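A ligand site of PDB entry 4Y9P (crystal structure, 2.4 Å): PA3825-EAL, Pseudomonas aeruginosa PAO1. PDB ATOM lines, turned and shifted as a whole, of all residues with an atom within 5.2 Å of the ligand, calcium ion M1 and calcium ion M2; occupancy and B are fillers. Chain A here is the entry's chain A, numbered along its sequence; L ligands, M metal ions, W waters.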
ATOM      1  N   GLN A  25      19.524 -20.043 -16.829  1.00  0.00           N
ATOM      2  CA  GLN A  25      18.628 -19.321 -15.937  1.00  0.00           C
ATOM      3  C   GLN A  25      19.349 -18.910 -14.615  1.00  0.00           C
ATOM      4  O   GLN A  25      19.822 -19.802 -13.841  1.00  0.00           O
ATOM      5  CB  GLN A  25      17.358 -20.136 -15.579  1.00  0.00           C
ATOM      6  CG  GLN A  25      16.374 -19.252 -14.788  1.00  0.00           C
ATOM      7  CD  GLN A  25      14.996 -19.842 -14.565  1.00  0.00           C
ATOM      8  OE1 GLN A  25      14.889 -21.009 -14.319  1.00  0.00           O
ATOM      9  NE2 GLN A  25      13.958 -19.008 -14.554  1.00  0.00           N
ATOM     10  N   GLU A  39      21.302 -22.282 -13.830  1.00  0.00           N
ATOM     11  CA  GLU A  39      20.875 -23.631 -14.269  1.00  0.00           C
ATOM     12  C   GLU A  39      20.974 -23.644 -15.755  1.00  0.00           C
ATOM     13  O   GLU A  39      20.485 -22.725 -16.402  1.00  0.00           O
ATOM     14  CB  GLU A  39      19.419 -23.979 -13.843  1.00  0.00           C
ATOM     15  CG  GLU A  39      19.060 -25.444 -14.109  1.00  0.00           C
ATOM     16  CD  GLU A  39      17.607 -25.847 -13.797  1.00  0.00           C
ATOM     17  OE1 GLU A  39      16.864 -24.999 -13.262  1.00  0.00           O
ATOM     18  OE2 GLU A  39      17.233 -27.044 -14.112  1.00  0.00           O
ATOM     19  N   VAL A  40      21.637 -24.653 -16.296  1.00  0.00           N
ATOM     20  CA  VAL A  40      21.786 -24.765 -17.698  1.00  0.00           C
ATOM     21  C   VAL A  40      20.595 -25.522 -18.191  1.00  0.00           C
ATOM     22  O   VAL A  40      20.368 -26.657 -17.703  1.00  0.00           O
ATOM     23  CB  VAL A  40      23.041 -25.588 -18.050  1.00  0.00           C
ATOM     24  CG1 VAL A  40      23.071 -25.883 -19.535  1.00  0.00           C
ATOM     25  CG2 VAL A  40      24.252 -24.826 -17.566  1.00  0.00           C
ATOM     26  N   LEU A  41      19.835 -24.924 -19.100  1.00  0.00           N
ATOM     27  CA  LEU A  41      18.641 -25.578 -19.691  1.00  0.00           C
ATOM     28  C   LEU A  41      18.812 -25.854 -21.200  1.00  0.00           C
ATOM     29  O   LEU A  41      19.226 -24.986 -21.949  1.00  0.00           O
ATOM     30  CB  LEU A  41      17.410 -24.690 -19.479  1.00  0.00           C
ATOM     31  CG  LEU A  41      16.665 -24.542 -18.158  1.00  0.00           C
ATOM     32  CD1 LEU A  41      17.297 -25.277 -17.010  1.00  0.00           C
ATOM     33  CD2 LEU A  41      16.527 -23.069 -17.844  1.00  0.00           C
ATOM     34  N   MET A  42      18.514 -27.060 -21.631  1.00  0.00           N
ATOM     35  CA  MET A  42      18.712 -27.391 -23.008  1.00  0.00           C
ATOM     36  C   MET A  42      17.681 -26.745 -23.904  1.00  0.00           C
ATOM     37  O   MET A  42      16.518 -26.633 -23.578  1.00  0.00           O
ATOM     38  CB  MET A  42      18.689 -28.889 -23.223  1.00  0.00           C
ATOM     39  CG  MET A  42      19.363 -29.294 -24.523  1.00  0.00           C
ATOM     40  SD  MET A  42      19.511 -31.116 -24.694  1.00  0.00           S
ATOM     41  CE  MET A  42      20.435 -31.604 -23.242  1.00  0.00           C
ATOM     42  N   ARG A  43      18.136 -26.325 -25.058  1.00  0.00           N
ATOM     43  CA  ARG A  43      17.260 -25.836 -26.085  1.00  0.00           C
ATOM     44  C   ARG A  43      17.678 -26.466 -27.360  1.00  0.00           C
ATOM     45  O   ARG A  43      18.873 -26.711 -27.583  1.00  0.00           O
ATOM     46  CB  ARG A  43      17.349 -24.299 -26.172  1.00  0.00           C
ATOM     47  CG  ARG A  43      16.767 -23.544 -24.975  1.00  0.00           C
ATOM     48  CD  ARG A  43      15.249 -23.591 -24.958  1.00  0.00           C
ATOM     49  NE  ARG A  43      14.654 -22.880 -23.813  1.00  0.00           N
ATOM     50  CZ  ARG A  43      14.511 -23.383 -22.575  1.00  0.00           C
ATOM     51  NH1 ARG A  43      14.898 -24.614 -22.278  1.00  0.00           N
ATOM     52  NH2 ARG A  43      13.924 -22.658 -21.630  1.00  0.00           N
ATOM     53  N   ARG A  53      11.472 -26.549 -27.257  1.00  0.00           N
ATOM     54  CA  ARG A  53      11.717 -26.664 -25.828  1.00  0.00           C
ATOM     55  C   ARG A  53      11.785 -28.114 -25.363  1.00  0.00           C
ATOM     56  O   ARG A  53      11.202 -29.004 -26.000  1.00  0.00           O
ATOM     57  CB  ARG A  53      10.663 -25.943 -25.070  1.00  0.00           C
ATOM     58  CG  ARG A  53      11.120 -24.639 -24.455  1.00  0.00           C
ATOM     59  CD  ARG A  53      10.009 -24.192 -23.506  1.00  0.00           C
ATOM     60  NE  ARG A  53      10.527 -23.466 -22.370  1.00  0.00           N
ATOM     61  CZ  ARG A  53       9.956 -23.361 -21.177  1.00  0.00           C
ATOM     62  NH1 ARG A  53       8.792 -23.938 -20.871  1.00  0.00           N
ATOM     63  NH2 ARG A  53      10.592 -22.645 -20.234  1.00  0.00           N
ATOM     64  N   PRO A  54      12.498 -28.350 -24.267  1.00  0.00           N
ATOM     65  CA  PRO A  54      12.866 -29.693 -23.765  1.00  0.00           C
ATOM     66  C   PRO A  54      11.789 -30.752 -23.675  1.00  0.00           C
ATOM     67  O   PRO A  54      12.050 -31.932 -23.974  1.00  0.00           O
ATOM     68  CB  PRO A  54      13.419 -29.429 -22.358  1.00  0.00           C
ATOM     69  CG  PRO A  54      13.869 -27.997 -22.366  1.00  0.00           C
ATOM     70  CD  PRO A  54      13.028 -27.277 -23.371  1.00  0.00           C
ATOM     71  N   ASP A  55      10.606 -30.357 -23.222  1.00  0.00           N
ATOM     72  CA  ASP A  55       9.538 -31.323 -22.973  1.00  0.00           C
ATOM     73  C   ASP A  55       9.060 -31.973 -24.236  1.00  0.00           C
ATOM     74  O   ASP A  55       8.548 -33.057 -24.172  1.00  0.00           O
ATOM     75  CB  ASP A  55       8.366 -30.700 -22.170  1.00  0.00           C
ATOM     76  CG  ASP A  55       8.769 -30.341 -20.699  1.00  0.00           C
ATOM     77  OD1 ASP A  55       9.793 -30.845 -20.160  1.00  0.00           O
ATOM     78  OD2 ASP A  55       8.050 -29.539 -20.078  1.00  0.00           O
ATOM     79  N   ILE A  58      13.293 -34.160 -24.700  1.00  0.00           N
ATOM     80  CA  ILE A  58      14.007 -34.903 -23.645  1.00  0.00           C
ATOM     81  C   ILE A  58      13.414 -36.283 -23.366  1.00  0.00           C
ATOM     82  O   ILE A  58      14.160 -37.242 -23.200  1.00  0.00           O
ATOM     83  CB  ILE A  58      14.125 -34.098 -22.331  1.00  0.00           C
ATOM     84  CG1 ILE A  58      15.081 -32.926 -22.498  1.00  0.00           C
ATOM     85  CG2 ILE A  58      14.593 -34.979 -21.179  1.00  0.00           C
ATOM     86  CD1 ILE A  58      16.537 -33.300 -22.665  1.00  0.00           C
ATOM     87  N   GLU A  62      15.794 -39.715 -23.580  1.00  0.00           N
ATOM     88  CA  GLU A  62      15.964 -40.613 -22.433  1.00  0.00           C
ATOM     89  C   GLU A  62      15.680 -42.046 -22.796  1.00  0.00           C
ATOM     90  O   GLU A  62      16.470 -42.903 -22.474  1.00  0.00           O
ATOM     91  CB  GLU A  62      15.137 -40.141 -21.217  1.00  0.00           C
ATOM     92  CG  GLU A  62      15.693 -38.832 -20.645  1.00  0.00           C
ATOM     93  CD  GLU A  62      14.954 -38.281 -19.436  1.00  0.00           C
ATOM     94  OE1 GLU A  62      13.734 -38.521 -19.279  1.00  0.00           O
ATOM     95  OE2 GLU A  62      15.602 -37.536 -18.640  1.00  0.00           O
ATOM     96  N   ILE A  67      20.272 -39.046 -24.582  1.00  0.00           N
ATOM     97  CA  ILE A  67      20.382 -37.962 -23.591  1.00  0.00           C
ATOM     98  C   ILE A  67      21.763 -37.881 -22.939  1.00  0.00           C
ATOM     99  O   ILE A  67      22.270 -36.786 -22.626  1.00  0.00           O
ATOM    100  CB  ILE A  67      19.271 -38.062 -22.516  1.00  0.00           C
ATOM    101  CG1 ILE A  67      19.251 -36.815 -21.618  1.00  0.00           C
ATOM    102  CG2 ILE A  67      19.421 -39.312 -21.668  1.00  0.00           C
ATOM    103  CD1 ILE A  67      19.038 -35.510 -22.364  1.00  0.00           C
ATOM    104  N   THR A  71      23.948 -34.512 -23.164  1.00  0.00           N
ATOM    105  CA  THR A  71      24.333 -33.796 -21.974  1.00  0.00           C
ATOM    106  C   THR A  71      25.841 -33.510 -21.975  1.00  0.00           C
ATOM    107  O   THR A  71      26.321 -32.445 -21.512  1.00  0.00           O
ATOM    108  CB  THR A  71      23.907 -34.643 -20.776  1.00  0.00           C
ATOM    109  OG1 THR A  71      22.499 -34.856 -20.861  1.00  0.00           O
ATOM    110  CG2 THR A  71      24.286 -33.999 -19.471  1.00  0.00           C
ATOM    111  N   LEU A  74      26.528 -30.591 -24.134  1.00  0.00           N
ATOM    112  CA  LEU A  74      26.047 -29.373 -23.455  1.00  0.00           C
ATOM    113  C   LEU A  74      27.080 -28.893 -22.440  1.00  0.00           C
ATOM    114  O   LEU A  74      27.436 -27.736 -22.434  1.00  0.00           O
ATOM    115  CB  LEU A  74      24.708 -29.658 -22.766  1.00  0.00           C
ATOM    116  CG  LEU A  74      23.851 -28.432 -22.492  1.00  0.00           C
ATOM    117  CD1 LEU A  74      23.212 -27.941 -23.793  1.00  0.00           C
ATOM    118  CD2 LEU A  74      22.784 -28.809 -21.463  1.00  0.00           C
ATOM    119  N   ASN A  98      20.890 -30.575 -15.539  1.00  0.00           N
ATOM    120  CA  ASN A  98      19.893 -31.582 -15.286  1.00  0.00           C
ATOM    121  C   ASN A  98      20.443 -32.917 -15.792  1.00  0.00           C
ATOM    122  O   ASN A  98      20.946 -32.973 -16.877  1.00  0.00           O
ATOM    123  CB  ASN A  98      18.592 -31.214 -16.015  1.00  0.00           C
ATOM    124  CG  ASN A  98      17.981 -29.977 -15.439  1.00  0.00           C
ATOM    125  OD1 ASN A  98      17.375 -30.037 -14.377  1.00  0.00           O
ATOM    126  ND2 ASN A  98      18.162 -28.837 -16.105  1.00  0.00           N
ATOM    127  N   ILE A  99      20.327 -33.980 -15.007  1.00  0.00           N
ATOM    128  CA  ILE A  99      20.944 -35.310 -15.268  1.00  0.00           C
ATOM    129  C   ILE A  99      19.834 -36.336 -15.303  1.00  0.00           C
ATOM    130  O   ILE A  99      18.941 -36.291 -14.483  1.00  0.00           O
ATOM    131  CB  ILE A  99      21.901 -35.619 -14.065  1.00  0.00           C
ATOM    132  CG1 ILE A  99      23.208 -34.795 -14.122  1.00  0.00           C
ATOM    133  CG2 ILE A  99      22.300 -37.064 -13.911  1.00  0.00           C
ATOM    134  CD1 ILE A  99      23.786 -34.542 -15.484  1.00  0.00           C
ATOM    135  N   SER A 100      19.886 -37.280 -16.238  1.00  0.00           N
ATOM    136  CA  SER A 100      18.913 -38.364 -16.299  1.00  0.00           C
ATOM    137  C   SER A 100      19.300 -39.571 -15.438  1.00  0.00           C
ATOM    138  O   SER A 100      20.428 -39.715 -15.013  1.00  0.00           O
ATOM    139  CB  SER A 100      18.643 -38.828 -17.741  1.00  0.00           C
ATOM    140  OG  SER A 100      19.793 -38.660 -18.511  1.00  0.00           O
ATOM    141  N   GLU A 130      21.460 -32.055 -10.993  1.00  0.00           N
ATOM    142  CA  GLU A 130      20.086 -32.073 -10.545  1.00  0.00           C
ATOM    143  C   GLU A 130      19.465 -33.351 -11.021  1.00  0.00           C
ATOM    144  O   GLU A 130      19.486 -33.682 -12.209  1.00  0.00           O
ATOM    145  CB  GLU A 130      19.301 -30.848 -11.044  1.00  0.00           C
ATOM    146  CG  GLU A 130      20.030 -29.530 -10.946  1.00  0.00           C
ATOM    147  CD  GLU A 130      19.143 -28.323 -11.245  1.00  0.00           C
ATOM    148  OE1 GLU A 130      17.985 -28.500 -11.713  1.00  0.00           O
ATOM    149  OE2 GLU A 130      19.600 -27.172 -10.967  1.00  0.00           O
ATOM    150  N   ASP A 160      15.857 -32.226  -7.807  1.00  0.00           N
ATOM    151  CA  ASP A 160      15.043 -31.336  -8.616  1.00  0.00           C
ATOM    152  C   ASP A 160      13.619 -31.605  -8.291  1.00  0.00           C
ATOM    153  O   ASP A 160      13.299 -32.708  -7.873  1.00  0.00           O
ATOM    154  CB  ASP A 160      15.252 -31.627 -10.082  1.00  0.00           C
ATOM    155  CG  ASP A 160      15.111 -30.425 -10.946  1.00  0.00           C
ATOM    156  OD1 ASP A 160      14.430 -29.457 -10.579  1.00  0.00           O
ATOM    157  OD2 ASP A 160      15.727 -30.459 -12.012  1.00  0.00           O
ATOM    158  N   ASP A 161      12.779 -30.604  -8.469  1.00  0.00           N
ATOM    159  CA  ASP A 161      11.300 -30.789  -8.347  1.00  0.00           C
ATOM    160  C   ASP A 161      10.892 -31.544  -7.084  1.00  0.00           C
ATOM    161  O   ASP A 161      10.094 -32.474  -7.131  1.00  0.00           O
ATOM    162  CB  ASP A 161      10.739 -31.466  -9.619  1.00  0.00           C
ATOM    163  CG  ASP A 161      11.062 -30.664 -10.913  1.00  0.00           C
ATOM    164  OD1 ASP A 161      11.230 -29.373 -10.933  1.00  0.00           O
ATOM    165  OD2 ASP A 161      11.143 -31.400 -11.923  1.00  0.00           O
ATOM    166  N   LYS A 181      15.826 -28.584  -4.490  1.00  0.00           N
ATOM    167  CA  LYS A 181      15.070 -27.575  -5.252  1.00  0.00           C
ATOM    168  C   LYS A 181      13.568 -27.760  -5.138  1.00  0.00           C
ATOM    169  O   LYS A 181      12.974 -28.751  -5.569  1.00  0.00           O
ATOM    170  CB  LYS A 181      15.481 -27.620  -6.696  1.00  0.00           C
ATOM    171  CG  LYS A 181      16.978 -27.517  -6.820  1.00  0.00           C
ATOM    172  CD  LYS A 181      17.415 -27.313  -8.253  1.00  0.00           C
ATOM    173  CE  LYS A 181      17.226 -25.915  -8.739  1.00  0.00           C
ATOM    174  NZ  LYS A 181      17.288 -25.861 -10.205  1.00  0.00           N
ATOM    175  N   ASP A 183      10.062 -27.631  -6.078  1.00  0.00           N
ATOM    176  CA  ASP A 183       9.266 -27.472  -7.314  1.00  0.00           C
ATOM    177  C   ASP A 183       8.405 -26.189  -7.365  1.00  0.00           C
ATOM    178  O   ASP A 183       7.777 -25.766  -6.357  1.00  0.00           O
ATOM    179  CB  ASP A 183       8.327 -28.644  -7.469  1.00  0.00           C
ATOM    180  CG  ASP A 183       7.727 -28.722  -8.861  1.00  0.00           C
ATOM    181  OD1 ASP A 183       8.503 -28.942  -9.824  1.00  0.00           O
ATOM    182  OD2 ASP A 183       6.492 -28.579  -8.941  1.00  0.00           O
ATOM    183  N   GLN A 184       8.278 -25.654  -8.551  1.00  0.00           N
ATOM    184  CA  GLN A 184       7.426 -24.471  -8.785  1.00  0.00           C
ATOM    185  C   GLN A 184       5.975 -24.609  -8.405  1.00  0.00           C
ATOM    186  O   GLN A 184       5.307 -23.612  -8.118  1.00  0.00           O
ATOM    187  CB  GLN A 184       7.575 -23.943 -10.231  1.00  0.00           C
ATOM    188  CG  GLN A 184       7.838 -24.963 -11.354  1.00  0.00           C
ATOM    189  CD  GLN A 184       8.407 -24.370 -12.641  1.00  0.00           C
ATOM    190  OE1 GLN A 184       7.651 -24.109 -13.574  1.00  0.00           O
ATOM    191  NE2 GLN A 184       9.754 -24.143 -12.712  1.00  0.00           N
ATOM    192  N   GLU A 217      12.247 -22.670  -6.878  1.00  0.00           N
ATOM    193  CA  GLU A 217      12.039 -22.524  -8.342  1.00  0.00           C
ATOM    194  C   GLU A 217      10.694 -21.909  -8.643  1.00  0.00           C
ATOM    195  O   GLU A 217       9.772 -22.091  -7.919  1.00  0.00           O
ATOM    196  CB  GLU A 217      11.993 -23.887  -9.021  1.00  0.00           C
ATOM    197  CG  GLU A 217      13.248 -24.744  -8.960  1.00  0.00           C
ATOM    198  CD  GLU A 217      12.959 -26.094  -9.697  1.00  0.00           C
ATOM    199  OE1 GLU A 217      12.582 -26.111 -10.903  1.00  0.00           O
ATOM    200  OE2 GLU A 217      12.997 -27.184  -9.061  1.00  0.00           O
ATOM    201  N   GLY A 218      10.609 -21.134  -9.708  1.00  0.00           N
ATOM    202  CA  GLY A 218       9.378 -20.526 -10.151  1.00  0.00           C
ATOM    203  C   GLY A 218       8.934 -19.344  -9.331  1.00  0.00           C
ATOM    204  O   GLY A 218       7.738 -19.052  -9.253  1.00  0.00           O
ATOM    205  N   VAL A 219       9.872 -18.594  -8.770  1.00  0.00           N
ATOM    206  CA  VAL A 219       9.503 -17.343  -8.080  1.00  0.00           C
ATOM    207  C   VAL A 219       9.161 -16.284  -9.146  1.00  0.00           C
ATOM    208  O   VAL A 219       9.992 -15.933  -9.950  1.00  0.00           O
ATOM    209  CB  VAL A 219      10.673 -16.838  -7.240  1.00  0.00           C
ATOM    210  CG1 VAL A 219      10.318 -15.570  -6.487  1.00  0.00           C
ATOM    211  CG2 VAL A 219      11.097 -17.901  -6.296  1.00  0.00           C
ATOM    212  N   GLU A 220       7.936 -15.884  -9.191  1.00  0.00           N
ATOM    213  CA  GLU A 220       7.436 -14.889 -10.138  1.00  0.00           C
ATOM    214  C   GLU A 220       6.959 -13.592  -9.487  1.00  0.00           C
ATOM    215  O   GLU A 220       6.908 -12.561 -10.137  1.00  0.00           O
ATOM    216  CB  GLU A 220       6.225 -15.487 -10.918  1.00  0.00           C
ATOM    217  CG  GLU A 220       6.594 -16.752 -11.636  1.00  0.00           C
ATOM    218  CD  GLU A 220       5.423 -17.436 -12.314  1.00  0.00           C
ATOM    219  OE1 GLU A 220       4.228 -17.147 -12.035  1.00  0.00           O
ATOM    220  OE2 GLU A 220       5.708 -18.353 -13.117  1.00  0.00           O
ATOM    221  N   GLN A 237      14.937 -18.774  -7.907  1.00  0.00           N
ATOM    222  CA  GLN A 237      15.034 -18.968  -9.335  1.00  0.00           C
ATOM    223  C   GLN A 237      13.631 -18.774  -9.867  1.00  0.00           C
ATOM    224  O   GLN A 237      12.627 -19.187  -9.247  1.00  0.00           O
ATOM    225  CB  GLN A 237      15.620 -20.358  -9.565  1.00  0.00           C
ATOM    226  CG  GLN A 237      15.687 -20.786 -10.961  1.00  0.00           C
ATOM    227  CD  GLN A 237      16.320 -22.174 -11.138  1.00  0.00           C
ATOM    228  OE1 GLN A 237      16.769 -22.849 -10.181  1.00  0.00           O
ATOM    229  NE2 GLN A 237      16.415 -22.587 -12.408  1.00  0.00           N
ATOM    230  N   GLY A 238      13.539 -18.089 -10.987  1.00  0.00           N
ATOM    231  CA  GLY A 238      12.206 -17.859 -11.566  1.00  0.00           C
ATOM    232  C   GLY A 238      12.219 -16.609 -12.430  1.00  0.00           C
ATOM    233  O   GLY A 238      13.221 -15.890 -12.442  1.00  0.00           O
ATOM    234  N   TYR A 239      11.067 -16.319 -13.090  1.00  0.00           N
ATOM    235  CA  TYR A 239      10.893 -15.136 -13.904  1.00  0.00           C
ATOM    236  C   TYR A 239      11.107 -13.868 -13.132  1.00  0.00           C
ATOM    237  O   TYR A 239      11.508 -12.932 -13.749  1.00  0.00           O
ATOM    238  CB  TYR A 239       9.529 -15.107 -14.626  1.00  0.00           C
ATOM    239  CG  TYR A 239       9.363 -16.288 -15.627  1.00  0.00           C
ATOM    240  CD1 TYR A 239      10.473 -16.949 -16.171  1.00  0.00           C
ATOM    241  CD2 TYR A 239       8.137 -16.784 -15.958  1.00  0.00           C
ATOM    242  CE1 TYR A 239      10.338 -17.978 -17.055  1.00  0.00           C
ATOM    243  CE2 TYR A 239       8.005 -17.831 -16.854  1.00  0.00           C
ATOM    244  CZ  TYR A 239       9.129 -18.412 -17.415  1.00  0.00           C
ATOM    245  OH  TYR A 239       9.115 -19.490 -18.302  1.00  0.00           O
ATOM    246  N   LEU A 240      10.893 -13.865 -11.809  1.00  0.00           N
ATOM    247  CA  LEU A 240      11.175 -12.683 -11.009  1.00  0.00           C
ATOM    248  C   LEU A 240      12.650 -12.304 -11.080  1.00  0.00           C
ATOM    249  O   LEU A 240      12.958 -11.166 -11.192  1.00  0.00           O
ATOM    250  CB  LEU A 240      10.745 -12.845  -9.547  1.00  0.00           C
ATOM    251  CG  LEU A 240      10.746 -11.494  -8.739  1.00  0.00           C
ATOM    252  CD1 LEU A 240       9.387 -10.885  -8.568  1.00  0.00           C
ATOM    253  CD2 LEU A 240      11.273 -11.636  -7.346  1.00  0.00           C
ATOM    254  N   PRO A 244      15.247 -18.012 -18.518  1.00  0.00           N
ATOM    255  CA  PRO A 244      16.311 -18.734 -19.199  1.00  0.00           C
ATOM    256  C   PRO A 244      16.749 -17.908 -20.369  1.00  0.00           C
ATOM    257  O   PRO A 244      15.907 -17.321 -20.983  1.00  0.00           O
ATOM    258  CB  PRO A 244      15.636 -19.989 -19.694  1.00  0.00           C
ATOM    259  CG  PRO A 244      14.464 -20.183 -18.818  1.00  0.00           C
ATOM    260  CD  PRO A 244      14.034 -18.820 -18.365  1.00  0.00           C
HETATM  261  P1  LIG L   1      13.132 -28.227 -14.497  1.00  0.00           P
HETATM  262  O1  LIG L   1      14.594 -28.500 -14.617  1.00  0.00           O
HETATM  263  O2  LIG L   1      12.418 -28.723 -13.256  1.00  0.00           O
HETATM  264  O3  LIG L   1      12.663 -26.723 -14.418  1.00  0.00           O
HETATM  265  C1  LIG L   1      13.092 -25.705 -15.255  1.00  0.00           C
HETATM  266  C2  LIG L   1      11.862 -25.332 -16.059  1.00  0.00           C
HETATM  267  O4  LIG L   1      11.013 -24.317 -15.504  1.00  0.00           O
HETATM  268  C3  LIG L   1      12.368 -24.748 -17.336  1.00  0.00           C
HETATM  269  O5  LIG L   1      11.535 -25.150 -18.413  1.00  0.00           O
HETATM  270  C4  LIG L   1      12.281 -23.291 -17.086  1.00  0.00           C
HETATM  271  O6  LIG L   1      12.304 -22.611 -18.310  1.00  0.00           O
HETATM  272  C5  LIG L   1      10.961 -23.193 -16.378  1.00  0.00           C
HETATM  273  N1  LIG L   1      10.809 -22.000 -15.547  1.00  0.00           N
HETATM  274  C6  LIG L   1      11.777 -21.290 -14.973  1.00  0.00           C
HETATM  275  N2  LIG L   1      11.307 -20.291 -14.206  1.00  0.00           N
HETATM  276  C7  LIG L   1      10.011 -20.339 -14.297  1.00  0.00           C
HETATM  277  C8  LIG L   1       8.941 -19.545 -13.729  1.00  0.00           C
HETATM  278  O7  LIG L   1       9.210 -18.581 -12.982  1.00  0.00           O
HETATM  279  N3  LIG L   1       7.708 -19.917 -14.041  1.00  0.00           N
HETATM  280  C9  LIG L   1       7.429 -20.978 -14.850  1.00  0.00           C
HETATM  281  N4  LIG L   1       6.138 -21.264 -15.114  1.00  0.00           N
HETATM  282  N5  LIG L   1       8.386 -21.764 -15.411  1.00  0.00           N
HETATM  283  C10 LIG L   1       9.670 -21.468 -15.180  1.00  0.00           C
HETATM  284  P2  LIG L   1      12.269 -25.764 -19.699  1.00  0.00           P
HETATM  285  O8  LIG L   1      13.569 -25.028 -20.012  1.00  0.00           O
HETATM  286  O9  LIG L   1      11.212 -26.025 -20.732  1.00  0.00           O
HETATM  287  O10 LIG L   1      12.704 -27.187 -19.081  1.00  0.00           O
HETATM  288  C11 LIG L   1      11.640 -28.043 -18.594  1.00  0.00           C
HETATM  289  C12 LIG L   1      12.226 -29.332 -18.072  1.00  0.00           C
HETATM  290  O11 LIG L   1      13.014 -29.955 -19.072  1.00  0.00           O
HETATM  291  C13 LIG L   1      13.186 -29.086 -16.950  1.00  0.00           C
HETATM  292  O12 LIG L   1      12.425 -28.834 -15.792  1.00  0.00           O
HETATM  293  C14 LIG L   1      14.001 -30.347 -17.012  1.00  0.00           C
HETATM  294  O13 LIG L   1      13.297 -31.427 -16.466  1.00  0.00           O
HETATM  295  C15 LIG L   1      14.099 -30.682 -18.480  1.00  0.00           C
HETATM  296  N6  LIG L   1      15.437 -30.340 -19.018  1.00  0.00           N
HETATM  297  C16 LIG L   1      15.881 -29.178 -19.542  1.00  0.00           C
HETATM  298  N7  LIG L   1      17.171 -29.288 -19.954  1.00  0.00           N
HETATM  299  C17 LIG L   1      17.540 -30.549 -19.667  1.00  0.00           C
HETATM  300  C18 LIG L   1      18.734 -31.357 -19.831  1.00  0.00           C
HETATM  301  O14 LIG L   1      19.735 -30.778 -20.323  1.00  0.00           O
HETATM  302  N8  LIG L   1      18.704 -32.660 -19.438  1.00  0.00           N
HETATM  303  C19 LIG L   1      17.621 -33.233 -18.890  1.00  0.00           C
HETATM  304  N9  LIG L   1      17.619 -34.522 -18.474  1.00  0.00           N
HETATM  305  N10 LIG L   1      16.490 -32.530 -18.720  1.00  0.00           N
HETATM  306  C20 LIG L   1      16.406 -31.233 -19.067  1.00  0.00           C
HETATM  307 CA    CA M   1      10.606 -27.323 -11.365  1.00  0.00          CA
HETATM  308 CA    CA M   2      16.096 -28.573 -13.043  1.00  0.00          CA
HETATM  309 CA    CA M   3      16.255 -34.570 -15.020  1.00  0.00          CA
HETATM  310  O   HOH W   1      21.021 -29.255 -17.881  1.00  0.00           O
HETATM  311  O   HOH W   2      15.291 -26.746 -11.891  1.00  0.00           O
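The side-chain carboxylate of Asp 161 sits close to an oxygen (O2) of the ligand (2.7 Å). A nitrogen (N8) of the ligand lies within hydrogen-bond range of the backbone carbonyl oxygen of Asn 98 (3.4 Å). The guanidinium group of Arg 53 is in salt-bridge range of an oxygen (O9) of the ligand (3.1 Å). NH1 of Arg 43 lies within salt-bridge range of O8 of the ligand. The side-chain carboxylate of Glu 220 lies within hydrogen-bond range of a nitrogen (N3) of the ligand, at 2.7 Å. N of Tyr 239 is in hydrogen-bond range of O7 of the ligand (2.9 Å). The side-chain amide nitrogen (NE2) of Gln 25 sits at hydrogen-bond distance from a nitrogen (N2) of the ligand, 3.0 Å away. An oxygen (O4) of the ligand lies within hydrogen-bond range of the side-chain amide nitrogen (NE2) of Gln 184, 3.1 Å away. The backbone NH (N) of Met 42 sits at hydrogen-bond distance from a nitrogen (N7) of the ligand (3.1 Å).
Of the 32 residues printed, 4 come within 4 Å of calcium ion M2. The nearest printed residue that does not touch calcium ion M2 is Lys 181 (4.1 Å).
Leu 41 touches the ligand. Pro 54 touches the ligand. Asp 55 touches the ligand. CD1 of Ile 58 touches C19 of the ligand, at 3.9 Å. Glu 62 touches the ligand (OE2 to N9, 3.6 Å). CD2 of Leu 74 touches O14 of the ligand, 3.8 Å away. Gly 218 touches the ligand. Gly 238 touches the ligand (CA to O7, 3.4 Å). CG of Pro 244 touches O6 of the ligand (3.3 Å). The nearest printed residue that does not touch the ligand is Ile 67 (4.1 Å).
Calcium ion M2 is bound by O1 of the ligand, OD2 of Asp 160, OE2 of Glu 39, water W2, OE1 of Glu 130 and OD1 of Asn 98. Slightly farther from calcium ion M2 lies OD1 of Asp 160 (3.1 Å).
Water W2 lies within hydrogen-bond range of the side-chain carboxylate of Glu 39, the side-chain amino group of Lys 181 and the side-chain carboxylate of Asp 160. Water W1 lies within hydrogen-bond range of O of Val 40 (2.7 Å), N of Asn 98 (2.7 Å) and O14 of the ligand (3.2 Å).
NE2 of Gln 184 touches calcium ion M1, 3.6 Å away. The nearest printed residue that does not touch calcium ion M1 is Asp 160 (4.4 Å).
Calcium ion M1 is bound by OD1 of Asp 161 (2.2 Å). OE1 of Glu 217 is bound to calcium ion M1, 2.4 Å away. Slightly farther from calcium ion M1 lies an oxygen (O2) of the ligand (3.0 Å). Slightly farther from calcium ion M1 lies the side-chain carboxylate (OD1) of Asp 183 (3.1 Å).
O of Glu 39 sits at hydrogen-bond distance from N of Gln 25 (2.9 Å). OE1 of Glu 39 is in hydrogen-bond range of NE2 of Gln 237, 2.6 Å away. The side-chain carboxylate of Glu 130 is in salt-bridge range of the side-chain amino group of Lys 181 (2.8 Å). O of Glu 130 lies within hydrogen-bond range of N of Ile 99, at 2.9 Å. ND2 of Asn 98 lies within hydrogen-bond range of O of Val 40. The backbone carbonyl oxygen (O) of Val 219 sits at hydrogen-bond distance from the backbone NH (N) of Tyr 239 (3.3 Å). OE1 of Gln 25 sits at hydrogen-bond distance from NE2 of Gln 237. The backbone NH (N) of Gly 218 lies within hydrogen-bond range of the backbone carbonyl oxygen (O) of Gln 237 (2.8 Å).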
